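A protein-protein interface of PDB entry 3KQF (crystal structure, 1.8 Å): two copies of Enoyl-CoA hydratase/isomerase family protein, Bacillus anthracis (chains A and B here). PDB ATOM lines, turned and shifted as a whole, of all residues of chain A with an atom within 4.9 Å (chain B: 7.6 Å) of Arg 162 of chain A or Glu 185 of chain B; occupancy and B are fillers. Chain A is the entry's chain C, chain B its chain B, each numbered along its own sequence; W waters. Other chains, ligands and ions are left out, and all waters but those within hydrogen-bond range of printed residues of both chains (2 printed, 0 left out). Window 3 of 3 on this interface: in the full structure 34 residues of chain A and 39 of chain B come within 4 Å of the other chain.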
ATOM      1  N   ILE A 158     -17.807 -35.837  27.786  1.00  0.00           N
ATOM      2  CA  ILE A 158     -17.495 -35.394  26.407  1.00  0.00           C
ATOM      3  C   ILE A 158     -16.652 -34.127  26.222  1.00  0.00           C
ATOM      4  O   ILE A 158     -16.410 -33.702  25.091  1.00  0.00           O
ATOM      5  CB  ILE A 158     -18.764 -35.284  25.567  1.00  0.00           C
ATOM      6  CG1 ILE A 158     -19.635 -34.096  25.971  1.00  0.00           C
ATOM      7  CG2 ILE A 158     -19.564 -36.600  25.600  1.00  0.00           C
ATOM      8  CD1 ILE A 158     -20.914 -34.002  25.158  1.00  0.00           C
ATOM      9  N   GLY A 159     -16.201 -33.534  27.307  1.00  0.00           N
ATOM     10  CA  GLY A 159     -15.385 -32.339  27.225  1.00  0.00           C
ATOM     11  C   GLY A 159     -16.257 -31.108  27.399  1.00  0.00           C
ATOM     12  O   GLY A 159     -17.453 -31.110  27.067  1.00  0.00           O
ATOM     13  N   VAL A 160     -15.656 -30.047  27.912  1.00  0.00           N
ATOM     14  CA  VAL A 160     -16.379 -28.820  28.177  1.00  0.00           C
ATOM     15  C   VAL A 160     -16.972 -28.161  26.947  1.00  0.00           C
ATOM     16  O   VAL A 160     -18.115 -27.704  26.984  1.00  0.00           O
ATOM     17  CB  VAL A 160     -15.484 -27.779  28.918  1.00  0.00           C
ATOM     18  CG1 VAL A 160     -15.255 -28.200  30.360  1.00  0.00           C
ATOM     19  CG2 VAL A 160     -14.145 -27.546  28.187  1.00  0.00           C
ATOM     20  N   GLY A 161     -16.205 -28.126  25.861  1.00  0.00           N
ATOM     21  CA  GLY A 161     -16.618 -27.443  24.641  1.00  0.00           C
ATOM     22  C   GLY A 161     -17.927 -27.972  24.091  1.00  0.00           C
ATOM     23  O   GLY A 161     -18.895 -27.228  23.866  1.00  0.00           O
ATOM     24  N   ARG A 162     -17.951 -29.268  23.875  1.00  0.00           N
ATOM     25  CA  ARG A 162     -19.154 -29.899  23.357  1.00  0.00           C
ATOM     26  C   ARG A 162     -20.325 -29.778  24.321  1.00  0.00           C
ATOM     27  O   ARG A 162     -21.457 -29.514  23.901  1.00  0.00           O
ATOM     28  CB  ARG A 162     -18.876 -31.350  23.015  1.00  0.00           C
ATOM     29  CG  ARG A 162     -20.027 -32.046  22.319  1.00  0.00           C
ATOM     30  CD  ARG A 162     -20.378 -31.373  20.978  1.00  0.00           C
ATOM     31  NE  ARG A 162     -19.309 -31.481  20.001  1.00  0.00           N
ATOM     32  CZ  ARG A 162     -19.325 -30.940  18.780  1.00  0.00           C
ATOM     33  NH1 ARG A 162     -20.346 -30.191  18.356  1.00  0.00           N
ATOM     34  NH2 ARG A 162     -18.294 -31.148  17.970  1.00  0.00           N
ATOM     35  N   ALA A 163     -20.062 -29.991  25.608  1.00  0.00           N
ATOM     36  CA  ALA A 163     -21.093 -29.890  26.633  1.00  0.00           C
ATOM     37  C   ALA A 163     -21.721 -28.501  26.626  1.00  0.00           C
ATOM     38  O   ALA A 163     -22.936 -28.376  26.689  1.00  0.00           O
ATOM     39  CB  ALA A 163     -20.527 -30.211  27.997  1.00  0.00           C
ATOM     40  N   LYS A 164     -20.883 -27.463  26.520  1.00  0.00           N
ATOM     41  CA  LYS A 164     -21.380 -26.092  26.464  1.00  0.00           C
ATOM     42  C   LYS A 164     -22.266 -25.817  25.233  1.00  0.00           C
ATOM     43  O   LYS A 164     -23.389 -25.280  25.361  1.00  0.00           O
ATOM     44  CB  LYS A 164     -20.207 -25.109  26.532  1.00  0.00           C
ATOM     45  CG  LYS A 164     -19.625 -24.966  27.926  1.00  0.00           C
ATOM     46  CD  LYS A 164     -18.426 -24.050  27.952  1.00  0.00           C
ATOM     47  CE  LYS A 164     -18.021 -23.684  29.349  1.00  0.00           C
ATOM     48  NZ  LYS A 164     -16.998 -22.569  29.398  1.00  0.00           N
ATOM     49  N   GLU A 165     -21.801 -26.191  24.047  1.00  0.00           N
ATOM     50  CA  GLU A 165     -22.606 -25.904  22.880  1.00  0.00           C
ATOM     51  C   GLU A 165     -23.945 -26.609  22.993  1.00  0.00           C
ATOM     52  O   GLU A 165     -24.981 -25.991  22.740  1.00  0.00           O
ATOM     53  CB  GLU A 165     -21.878 -26.187  21.550  1.00  0.00           C
ATOM     54  CG  GLU A 165     -21.648 -27.624  21.164  1.00  0.00           C
ATOM     55  CD  GLU A 165     -22.785 -28.264  20.324  1.00  0.00           C
ATOM     56  OE1 GLU A 165     -22.520 -29.357  19.787  1.00  0.00           O
ATOM     57  OE2 GLU A 165     -23.900 -27.694  20.166  1.00  0.00           O
ATOM     58  N   LEU A 166     -23.939 -27.850  23.484  1.00  0.00           N
ATOM     59  CA  LEU A 166     -25.189 -28.627  23.643  1.00  0.00           C
ATOM     60  C   LEU A 166     -26.171 -28.063  24.694  1.00  0.00           C
ATOM     61  O   LEU A 166     -27.387 -27.981  24.447  1.00  0.00           O
ATOM     62  CB  LEU A 166     -24.868 -30.077  23.973  1.00  0.00           C
ATOM     63  CG  LEU A 166     -24.257 -30.924  22.850  1.00  0.00           C
ATOM     64  CD1 LEU A 166     -23.927 -32.316  23.395  1.00  0.00           C
ATOM     65  CD2 LEU A 166     -25.210 -31.005  21.672  1.00  0.00           C
ATOM     66  N   ARG A 171     -30.082 -27.956  21.890  1.00  0.00           N
ATOM     67  CA  ARG A 171     -30.447 -28.652  20.681  1.00  0.00           C
ATOM     68  C   ARG A 171     -30.498 -30.176  20.813  1.00  0.00           C
ATOM     69  O   ARG A 171     -29.832 -30.775  21.665  1.00  0.00           O
ATOM     70  CB  ARG A 171     -29.511 -28.261  19.527  1.00  0.00           C
ATOM     71  CG  ARG A 171     -28.090 -28.835  19.611  1.00  0.00           C
ATOM     72  CD  ARG A 171     -27.203 -28.258  18.528  1.00  0.00           C
ATOM     73  NE  ARG A 171     -25.860 -28.861  18.529  1.00  0.00           N
ATOM     74  CZ  ARG A 171     -25.470 -29.876  17.754  1.00  0.00           C
ATOM     75  NH1 ARG A 171     -26.297 -30.427  16.867  1.00  0.00           N
ATOM     76  NH2 ARG A 171     -24.230 -30.343  17.857  1.00  0.00           N
ATOM     77  N   TYR A 181     -19.527 -37.524  19.234  1.00  0.00           N
ATOM     78  CA  TYR A 181     -19.126 -36.677  20.359  1.00  0.00           C
ATOM     79  C   TYR A 181     -18.674 -37.478  21.567  1.00  0.00           C
ATOM     80  O   TYR A 181     -18.090 -36.917  22.479  1.00  0.00           O
ATOM     81  CB  TYR A 181     -20.263 -35.720  20.807  1.00  0.00           C
ATOM     82  CG  TYR A 181     -20.931 -34.925  19.700  1.00  0.00           C
ATOM     83  CD1 TYR A 181     -20.221 -34.517  18.579  1.00  0.00           C
ATOM     84  CD2 TYR A 181     -22.258 -34.510  19.818  1.00  0.00           C
ATOM     85  CE1 TYR A 181     -20.827 -33.800  17.581  1.00  0.00           C
ATOM     86  CE2 TYR A 181     -22.868 -33.761  18.834  1.00  0.00           C
ATOM     87  CZ  TYR A 181     -22.149 -33.412  17.705  1.00  0.00           C
ATOM     88  OH  TYR A 181     -22.755 -32.679  16.699  1.00  0.00           O
ATOM     89  N   ALA B 107     -15.941 -18.583  19.363  1.00  0.00           N
ATOM     90  CA  ALA B 107     -14.817 -18.244  18.501  1.00  0.00           C
ATOM     91  C   ALA B 107     -15.151 -18.661  17.066  1.00  0.00           C
ATOM     92  O   ALA B 107     -15.420 -19.846  16.801  1.00  0.00           O
ATOM     93  CB  ALA B 107     -13.532 -18.965  18.961  1.00  0.00           C
ATOM     94  N   ILE B 109     -13.349 -18.941  13.854  1.00  0.00           N
ATOM     95  CA  ILE B 109     -11.948 -19.012  13.396  1.00  0.00           C
ATOM     96  C   ILE B 109     -11.875 -18.952  11.873  1.00  0.00           C
ATOM     97  O   ILE B 109     -12.089 -19.943  11.191  1.00  0.00           O
ATOM     98  CB  ILE B 109     -11.250 -20.258  13.955  1.00  0.00           C
ATOM     99  CG1 ILE B 109     -11.489 -20.367  15.469  1.00  0.00           C
ATOM    100  CG2 ILE B 109      -9.725 -20.214  13.688  1.00  0.00           C
ATOM    101  CD1 ILE B 109     -10.883 -21.611  16.129  1.00  0.00           C
ATOM    102  N   SER B 121      -8.890 -18.692  21.268  1.00  0.00           N
ATOM    103  CA  SER B 121      -9.973 -19.620  20.856  1.00  0.00           C
ATOM    104  C   SER B 121     -10.320 -20.622  21.960  1.00  0.00           C
ATOM    105  O   SER B 121     -11.488 -20.983  22.125  1.00  0.00           O
ATOM    106  CB  SER B 121      -9.630 -20.374  19.557  1.00  0.00           C
ATOM    107  OG  SER B 121      -8.668 -21.404  19.746  1.00  0.00           O
ATOM    108  N   CYS B 124     -12.616 -19.196  24.705  1.00  0.00           N
ATOM    109  CA  CYS B 124     -14.018 -19.077  24.296  1.00  0.00           C
ATOM    110  C   CYS B 124     -14.772 -20.355  24.704  1.00  0.00           C
ATOM    111  O   CYS B 124     -14.164 -21.423  24.927  1.00  0.00           O
ATOM    112  CB  CYS B 124     -14.126 -18.807  22.790  1.00  0.00           C
ATOM    113  SG  CYS B 124     -13.400 -17.227  22.302  1.00  0.00           S
ATOM    114  N   ASP B 125     -16.081 -20.237  24.843  1.00  0.00           N
ATOM    115  CA  ASP B 125     -16.916 -21.357  25.241  1.00  0.00           C
ATOM    116  C   ASP B 125     -16.856 -22.503  24.223  1.00  0.00           C
ATOM    117  O   ASP B 125     -16.722 -23.664  24.607  1.00  0.00           O
ATOM    118  CB  ASP B 125     -18.339 -20.902  25.529  1.00  0.00           C
ATOM    119  CG  ASP B 125     -18.430 -20.042  26.792  1.00  0.00           C
ATOM    120  OD1 ASP B 125     -18.627 -20.643  27.883  1.00  0.00           O
ATOM    121  OD2 ASP B 125     -18.223 -18.804  26.713  1.00  0.00           O
ATOM    122  N   PHE B 126     -16.955 -22.178  22.936  1.00  0.00           N
ATOM    123  CA  PHE B 126     -16.791 -23.175  21.897  1.00  0.00           C
ATOM    124  C   PHE B 126     -16.353 -22.492  20.610  1.00  0.00           C
ATOM    125  O   PHE B 126     -16.308 -21.247  20.524  1.00  0.00           O
ATOM    126  CB  PHE B 126     -17.979 -24.126  21.722  1.00  0.00           C
ATOM    127  CG  PHE B 126     -19.241 -23.461  21.317  1.00  0.00           C
ATOM    128  CD1 PHE B 126     -19.583 -23.365  19.991  1.00  0.00           C
ATOM    129  CD2 PHE B 126     -20.127 -22.994  22.273  1.00  0.00           C
ATOM    130  CE1 PHE B 126     -20.770 -22.786  19.615  1.00  0.00           C
ATOM    131  CE2 PHE B 126     -21.321 -22.404  21.898  1.00  0.00           C
ATOM    132  CZ  PHE B 126     -21.643 -22.307  20.575  1.00  0.00           C
ATOM    133  N   ARG B 127     -15.970 -23.312  19.645  1.00  0.00           N
ATOM    134  CA  ARG B 127     -15.355 -22.821  18.434  1.00  0.00           C
ATOM    135  C   ARG B 127     -15.969 -23.372  17.169  1.00  0.00           C
ATOM    136  O   ARG B 127     -16.348 -24.553  17.107  1.00  0.00           O
ATOM    137  CB  ARG B 127     -13.863 -23.244  18.465  1.00  0.00           C
ATOM    138  CG  ARG B 127     -13.017 -22.592  19.589  1.00  0.00           C
ATOM    139  CD  ARG B 127     -12.031 -23.594  20.255  1.00  0.00           C
ATOM    140  NE  ARG B 127     -12.777 -24.591  21.016  1.00  0.00           N
ATOM    141  CZ  ARG B 127     -13.249 -24.379  22.245  1.00  0.00           C
ATOM    142  NH1 ARG B 127     -13.958 -25.319  22.855  1.00  0.00           N
ATOM    143  NH2 ARG B 127     -13.020 -23.208  22.857  1.00  0.00           N
ATOM    144  N   ILE B 128     -16.096 -22.504  16.164  1.00  0.00           N
ATOM    145  CA  ILE B 128     -16.565 -22.897  14.834  1.00  0.00           C
ATOM    146  C   ILE B 128     -15.510 -22.363  13.878  1.00  0.00           C
ATOM    147  O   ILE B 128     -15.166 -21.181  13.923  1.00  0.00           O
ATOM    148  CB  ILE B 128     -17.973 -22.361  14.478  1.00  0.00           C
ATOM    149  CG1 ILE B 128     -18.309 -22.723  13.022  1.00  0.00           C
ATOM    150  CG2 ILE B 128     -18.052 -20.851  14.698  1.00  0.00           C
ATOM    151  CD1 ILE B 128     -19.737 -22.385  12.603  1.00  0.00           C
ATOM    152  N   ALA B 129     -14.996 -23.232  13.017  1.00  0.00           N
ATOM    153  CA  ALA B 129     -13.908 -22.867  12.126  1.00  0.00           C
ATOM    154  C   ALA B 129     -14.255 -22.969  10.658  1.00  0.00           C
ATOM    155  O   ALA B 129     -15.040 -23.817  10.263  1.00  0.00           O
ATOM    156  CB  ALA B 129     -12.685 -23.776  12.418  1.00  0.00           C
ATOM    157  N   LEU B 157      -9.648 -29.734  27.043  1.00  0.00           N
ATOM    158  CA  LEU B 157     -10.595 -29.903  25.939  1.00  0.00           C
ATOM    159  C   LEU B 157     -10.437 -31.183  25.116  1.00  0.00           C
ATOM    160  O   LEU B 157     -11.437 -31.843  24.821  1.00  0.00           O
ATOM    161  CB  LEU B 157     -10.507 -28.703  24.996  1.00  0.00           C
ATOM    162  CG  LEU B 157     -11.499 -28.594  23.848  1.00  0.00           C
ATOM    163  CD1 LEU B 157     -12.929 -28.489  24.383  1.00  0.00           C
ATOM    164  CD2 LEU B 157     -11.156 -27.395  22.931  1.00  0.00           C
ATOM    165  N   ILE B 158      -9.193 -31.549  24.763  1.00  0.00           N
ATOM    166  CA  ILE B 158      -8.964 -32.690  23.870  1.00  0.00           C
ATOM    167  C   ILE B 158      -8.220 -33.906  24.461  1.00  0.00           C
ATOM    168  O   ILE B 158      -7.927 -34.871  23.749  1.00  0.00           O
ATOM    169  CB  ILE B 158      -8.221 -32.209  22.583  1.00  0.00           C
ATOM    170  CG1 ILE B 158      -6.759 -31.850  22.868  1.00  0.00           C
ATOM    171  CG2 ILE B 158      -8.929 -31.008  21.958  1.00  0.00           C
ATOM    172  CD1 ILE B 158      -5.987 -31.469  21.575  1.00  0.00           C
ATOM    173  N   ALA B 175      -8.306 -27.464  10.135  1.00  0.00           N
ATOM    174  CA  ALA B 175      -9.595 -27.404  10.794  1.00  0.00           C
ATOM    175  C   ALA B 175     -10.214 -28.805  10.874  1.00  0.00           C
ATOM    176  O   ALA B 175     -10.882 -29.158  11.865  1.00  0.00           O
ATOM    177  CB  ALA B 175     -10.530 -26.471  10.011  1.00  0.00           C
ATOM    178  N   ALA B 178      -8.526 -30.707  13.601  1.00  0.00           N
ATOM    179  CA  ALA B 178      -9.011 -30.091  14.847  1.00  0.00           C
ATOM    180  C   ALA B 178     -10.417 -30.610  15.210  1.00  0.00           C
ATOM    181  O   ALA B 178     -10.720 -30.856  16.386  1.00  0.00           O
ATOM    182  CB  ALA B 178      -8.990 -28.556  14.715  1.00  0.00           C
ATOM    183  N   LYS B 179     -11.264 -30.780  14.203  1.00  0.00           N
ATOM    184  CA  LYS B 179     -12.605 -31.291  14.399  1.00  0.00           C
ATOM    185  C   LYS B 179     -12.522 -32.730  14.907  1.00  0.00           C
ATOM    186  O   LYS B 179     -13.227 -33.110  15.839  1.00  0.00           O
ATOM    187  CB  LYS B 179     -13.400 -31.244  13.109  1.00  0.00           C
ATOM    188  CG  LYS B 179     -14.886 -31.531  13.302  1.00  0.00           C
ATOM    189  CD  LYS B 179     -15.661 -31.381  11.999  1.00  0.00           C
ATOM    190  CE  LYS B 179     -15.784 -32.649  11.232  1.00  0.00           C
ATOM    191  NZ  LYS B 179     -16.816 -33.529  11.852  1.00  0.00           N
ATOM    192  N   GLY B 182     -11.616 -32.753  18.514  1.00  0.00           N
ATOM    193  CA  GLY B 182     -12.560 -32.049  19.380  1.00  0.00           C
ATOM    194  C   GLY B 182     -12.023 -30.690  19.814  1.00  0.00           C
ATOM    195  O   GLY B 182     -12.522 -30.107  20.785  1.00  0.00           O
ATOM    196  N   LEU B 183     -11.011 -30.191  19.095  1.00  0.00           N
ATOM    197  CA  LEU B 183     -10.428 -28.847  19.352  1.00  0.00           C
ATOM    198  C   LEU B 183     -11.414 -27.771  18.838  1.00  0.00           C
ATOM    199  O   LEU B 183     -11.508 -26.704  19.422  1.00  0.00           O
ATOM    200  CB  LEU B 183      -9.073 -28.688  18.687  1.00  0.00           C
ATOM    201  CG  LEU B 183      -8.381 -27.315  18.765  1.00  0.00           C
ATOM    202  CD1 LEU B 183      -8.217 -26.797  20.195  1.00  0.00           C
ATOM    203  CD2 LEU B 183      -7.032 -27.380  18.069  1.00  0.00           C
ATOM    204  N   VAL B 184     -12.090 -28.039  17.714  1.00  0.00           N
ATOM    205  CA  VAL B 184     -13.151 -27.148  17.218  1.00  0.00           C
ATOM    206  C   VAL B 184     -14.404 -28.005  17.144  1.00  0.00           C
ATOM    207  O   VAL B 184     -14.357 -29.162  16.716  1.00  0.00           O
ATOM    208  CB  VAL B 184     -12.865 -26.455  15.837  1.00  0.00           C
ATOM    209  CG1 VAL B 184     -11.579 -25.642  15.919  1.00  0.00           C
ATOM    210  CG2 VAL B 184     -12.837 -27.444  14.718  1.00  0.00           C
ATOM    211  N   GLU B 185     -15.520 -27.428  17.559  1.00  0.00           N
ATOM    212  CA  GLU B 185     -16.806 -28.123  17.582  1.00  0.00           C
ATOM    213  C   GLU B 185     -17.527 -28.196  16.251  1.00  0.00           C
ATOM    214  O   GLU B 185     -18.334 -29.115  16.020  1.00  0.00           O
ATOM    215  CB  GLU B 185     -17.703 -27.466  18.631  1.00  0.00           C
ATOM    216  CG  GLU B 185     -17.286 -27.752  20.106  1.00  0.00           C
ATOM    217  CD  GLU B 185     -15.985 -27.084  20.582  1.00  0.00           C
ATOM    218  OE1 GLU B 185     -15.559 -26.048  20.028  1.00  0.00           O
ATOM    219  OE2 GLU B 185     -15.412 -27.576  21.585  1.00  0.00           O
ATOM    220  N   PHE B 186     -17.289 -27.213  15.383  1.00  0.00           N
ATOM    221  CA  PHE B 186     -17.922 -27.193  14.071  1.00  0.00           C
ATOM    222  C   PHE B 186     -16.953 -26.689  13.026  1.00  0.00           C
ATOM    223  O   PHE B 186     -16.104 -25.849  13.322  1.00  0.00           O
ATOM    224  CB  PHE B 186     -19.141 -26.248  14.058  1.00  0.00           C
ATOM    225  CG  PHE B 186     -20.167 -26.555  15.101  1.00  0.00           C
ATOM    226  CD1 PHE B 186     -21.150 -27.494  14.863  1.00  0.00           C
ATOM    227  CD2 PHE B 186     -20.168 -25.884  16.305  1.00  0.00           C
ATOM    228  CE1 PHE B 186     -22.110 -27.770  15.837  1.00  0.00           C
ATOM    229  CE2 PHE B 186     -21.121 -26.150  17.269  1.00  0.00           C
ATOM    230  CZ  PHE B 186     -22.084 -27.097  17.034  1.00  0.00           C
ATOM    231  N   VAL B 187     -17.078 -27.211  11.812  1.00  0.00           N
ATOM    232  CA  VAL B 187     -16.302 -26.739  10.661  1.00  0.00           C
ATOM    233  C   VAL B 187     -17.269 -26.528   9.500  1.00  0.00           C
ATOM    234  O   VAL B 187     -18.090 -27.394   9.216  1.00  0.00           O
ATOM    235  CB  VAL B 187     -15.170 -27.690  10.221  1.00  0.00           C
ATOM    236  CG1 VAL B 187     -14.508 -27.166   8.922  1.00  0.00           C
ATOM    237  CG2 VAL B 187     -14.148 -27.841  11.348  1.00  0.00           C
ATOM    238  N   ILE B 200     -26.067 -20.157  15.150  1.00  0.00           N
ATOM    239  CA  ILE B 200     -25.928 -20.802  16.459  1.00  0.00           C
ATOM    240  C   ILE B 200     -26.151 -19.789  17.589  1.00  0.00           C
ATOM    241  O   ILE B 200     -26.816 -20.091  18.582  1.00  0.00           O
ATOM    242  CB  ILE B 200     -24.539 -21.479  16.613  1.00  0.00           C
ATOM    243  CG1 ILE B 200     -24.369 -22.597  15.563  1.00  0.00           C
ATOM    244  CG2 ILE B 200     -24.395 -22.040  18.038  1.00  0.00           C
ATOM    245  CD1 ILE B 200     -22.949 -23.189  15.485  1.00  0.00           C
ATOM    246  N   ILE B 219     -21.188 -25.205  34.643  1.00  0.00           N
ATOM    247  CA  ILE B 219     -20.243 -26.009  33.892  1.00  0.00           C
ATOM    248  C   ILE B 219     -18.775 -25.573  34.121  1.00  0.00           C
ATOM    249  O   ILE B 219     -17.902 -26.407  34.410  1.00  0.00           O
ATOM    250  CB  ILE B 219     -20.531 -25.916  32.387  1.00  0.00           C
ATOM    251  CG1 ILE B 219     -21.901 -26.496  32.058  1.00  0.00           C
ATOM    252  CG2 ILE B 219     -19.421 -26.658  31.590  1.00  0.00           C
ATOM    253  CD1 ILE B 219     -22.409 -26.160  30.637  1.00  0.00           C
HETATM  254  O   HOH W   1     -15.416 -31.803  16.973  1.00  0.00           O
HETATM  255  O   HOH W   2     -15.166 -20.324  28.146  1.00  0.00           O
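Of the printed residues of chain B, Arg 162 of chain A touches Glu 185 (2.8 Å) and Phe 186 (3.8 Å). Printed residues of chain A within 4 Å of Glu 185 of chain B: Gly 161 (3.3 Å) and Arg 162 (2.8 Å). Gly 161 of chain A touches just these residues of chain B: Asp 125 (3.8 Å), Phe 126 (3.9 Å), Arg 127 (3.8 Å), Leu 157 (3.6 Å) and Glu 185 (3.3 Å). Of the printed residues of chain B, Glu 165 of chain A touches Phe 126 (3.7 Å) and Phe 186 (3.6 Å). Of the printed residues of chain A, Phe 186 of chain B touches Arg 162, Glu 165 and Arg 171. Of the printed residues of chain B, Lys 164 of chain A touches Asp 125 and Ile 219. Printed residues of chain A within 4 Å of Phe 126 of chain B: Gly 161 and Glu 165. Printed residues of chain A within 4 Å of Ile 219 of chain B: Lys 164. The nearest residue of chain B that does not touch Arg 162 of chain A is Val 184 of chain B (4.6 Å). The nearest residue of chain A that does not touch Glu 185 of chain B is Glu 165 of chain A (4.5 Å).
Water W1 lies within hydrogen-bond range of O of Lys 179 of chain B, O of Val 184 of chain B and NH2 of Arg 162 of chain A. Water W2 lies within hydrogen-bond range of NZ of Lys 164 of chain A (3.2 Å) and N of Asp 125 of chain B (3.4 Å).
Of the 11 printed residues of chain A, 5 touch a printed residue of chain B. Printed residues of chain A that touch a printed residue of chain B: Gly 161, Arg 162, Lys 164, Glu 165 and Arg 171. Of the 22 printed residues of chain B, 7 touch a printed residue of chain A. Among the printed residues, Asp or Glu carboxylates within 4 Å of a Lys or Arg side-chain nitrogen of the other chain: Lys 164 of chain A with Asp 125 of chain B (2.9 Å).
Among the printed residues, pairs that only touch across the chains: Gly 161 of chain A with Glu 185 of chain B, Glu 165 of chain A with Phe 186 of chain B, Gly 161 of chain A with Leu 157 of chain B, Glu 165 of chain A with Phe 126 of chain B, Gly 161 of chain A with Asp 125 of chain B, Arg 162 of chain A with Phe 186 of chain B, Gly 161 of chain A with Arg 127 of chain B, Gly 161 of chain A with Phe 126 of chain B, Arg 171 of chain A with Phe 186 of chain B and Lys 164 of chain A with Ile 219 of chain B.
Position printed for both chains: 158. Of the 12 pairs that touch across the chains among the printed residues, none has its exchanged pair printed and touching as well.
N of Ala 107 of chain B is in hydrogen-bond range of O of Phe 126 of chain B (2.9 Å). OE2 of Glu 185 of chain B is in salt-bridge range of NH1 of Arg 127 of chain B (3.0 Å). The backbone NH (N) of Phe 186 of chain B is in hydrogen-bond range of the backbone carbonyl oxygen (O) of Arg 127 of chain B. The backbone carbonyl oxygen (O) of Phe 186 of chain B lies within hydrogen-bond range of the backbone NH (N) of Ala 129 of chain B, 2.9 Å away. NH1 of Arg 162 of chain A lies within salt-bridge range of OE1 of Glu 165 of chain A (2.7 Å). The guanidinium group (NH2) of Arg 171 of chain A is in salt-bridge range of the side-chain carboxylate (OE1) of Glu 165 of chain A, 2.8 Å away.
OD1 of Asp 125 of chain B lies within salt-bridge range of NZ of Lys 164 of chain A. O of Glu 185 of chain B is in hydrogen-bond range of NH2 of Arg 162 of chain A (2.8 Å).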
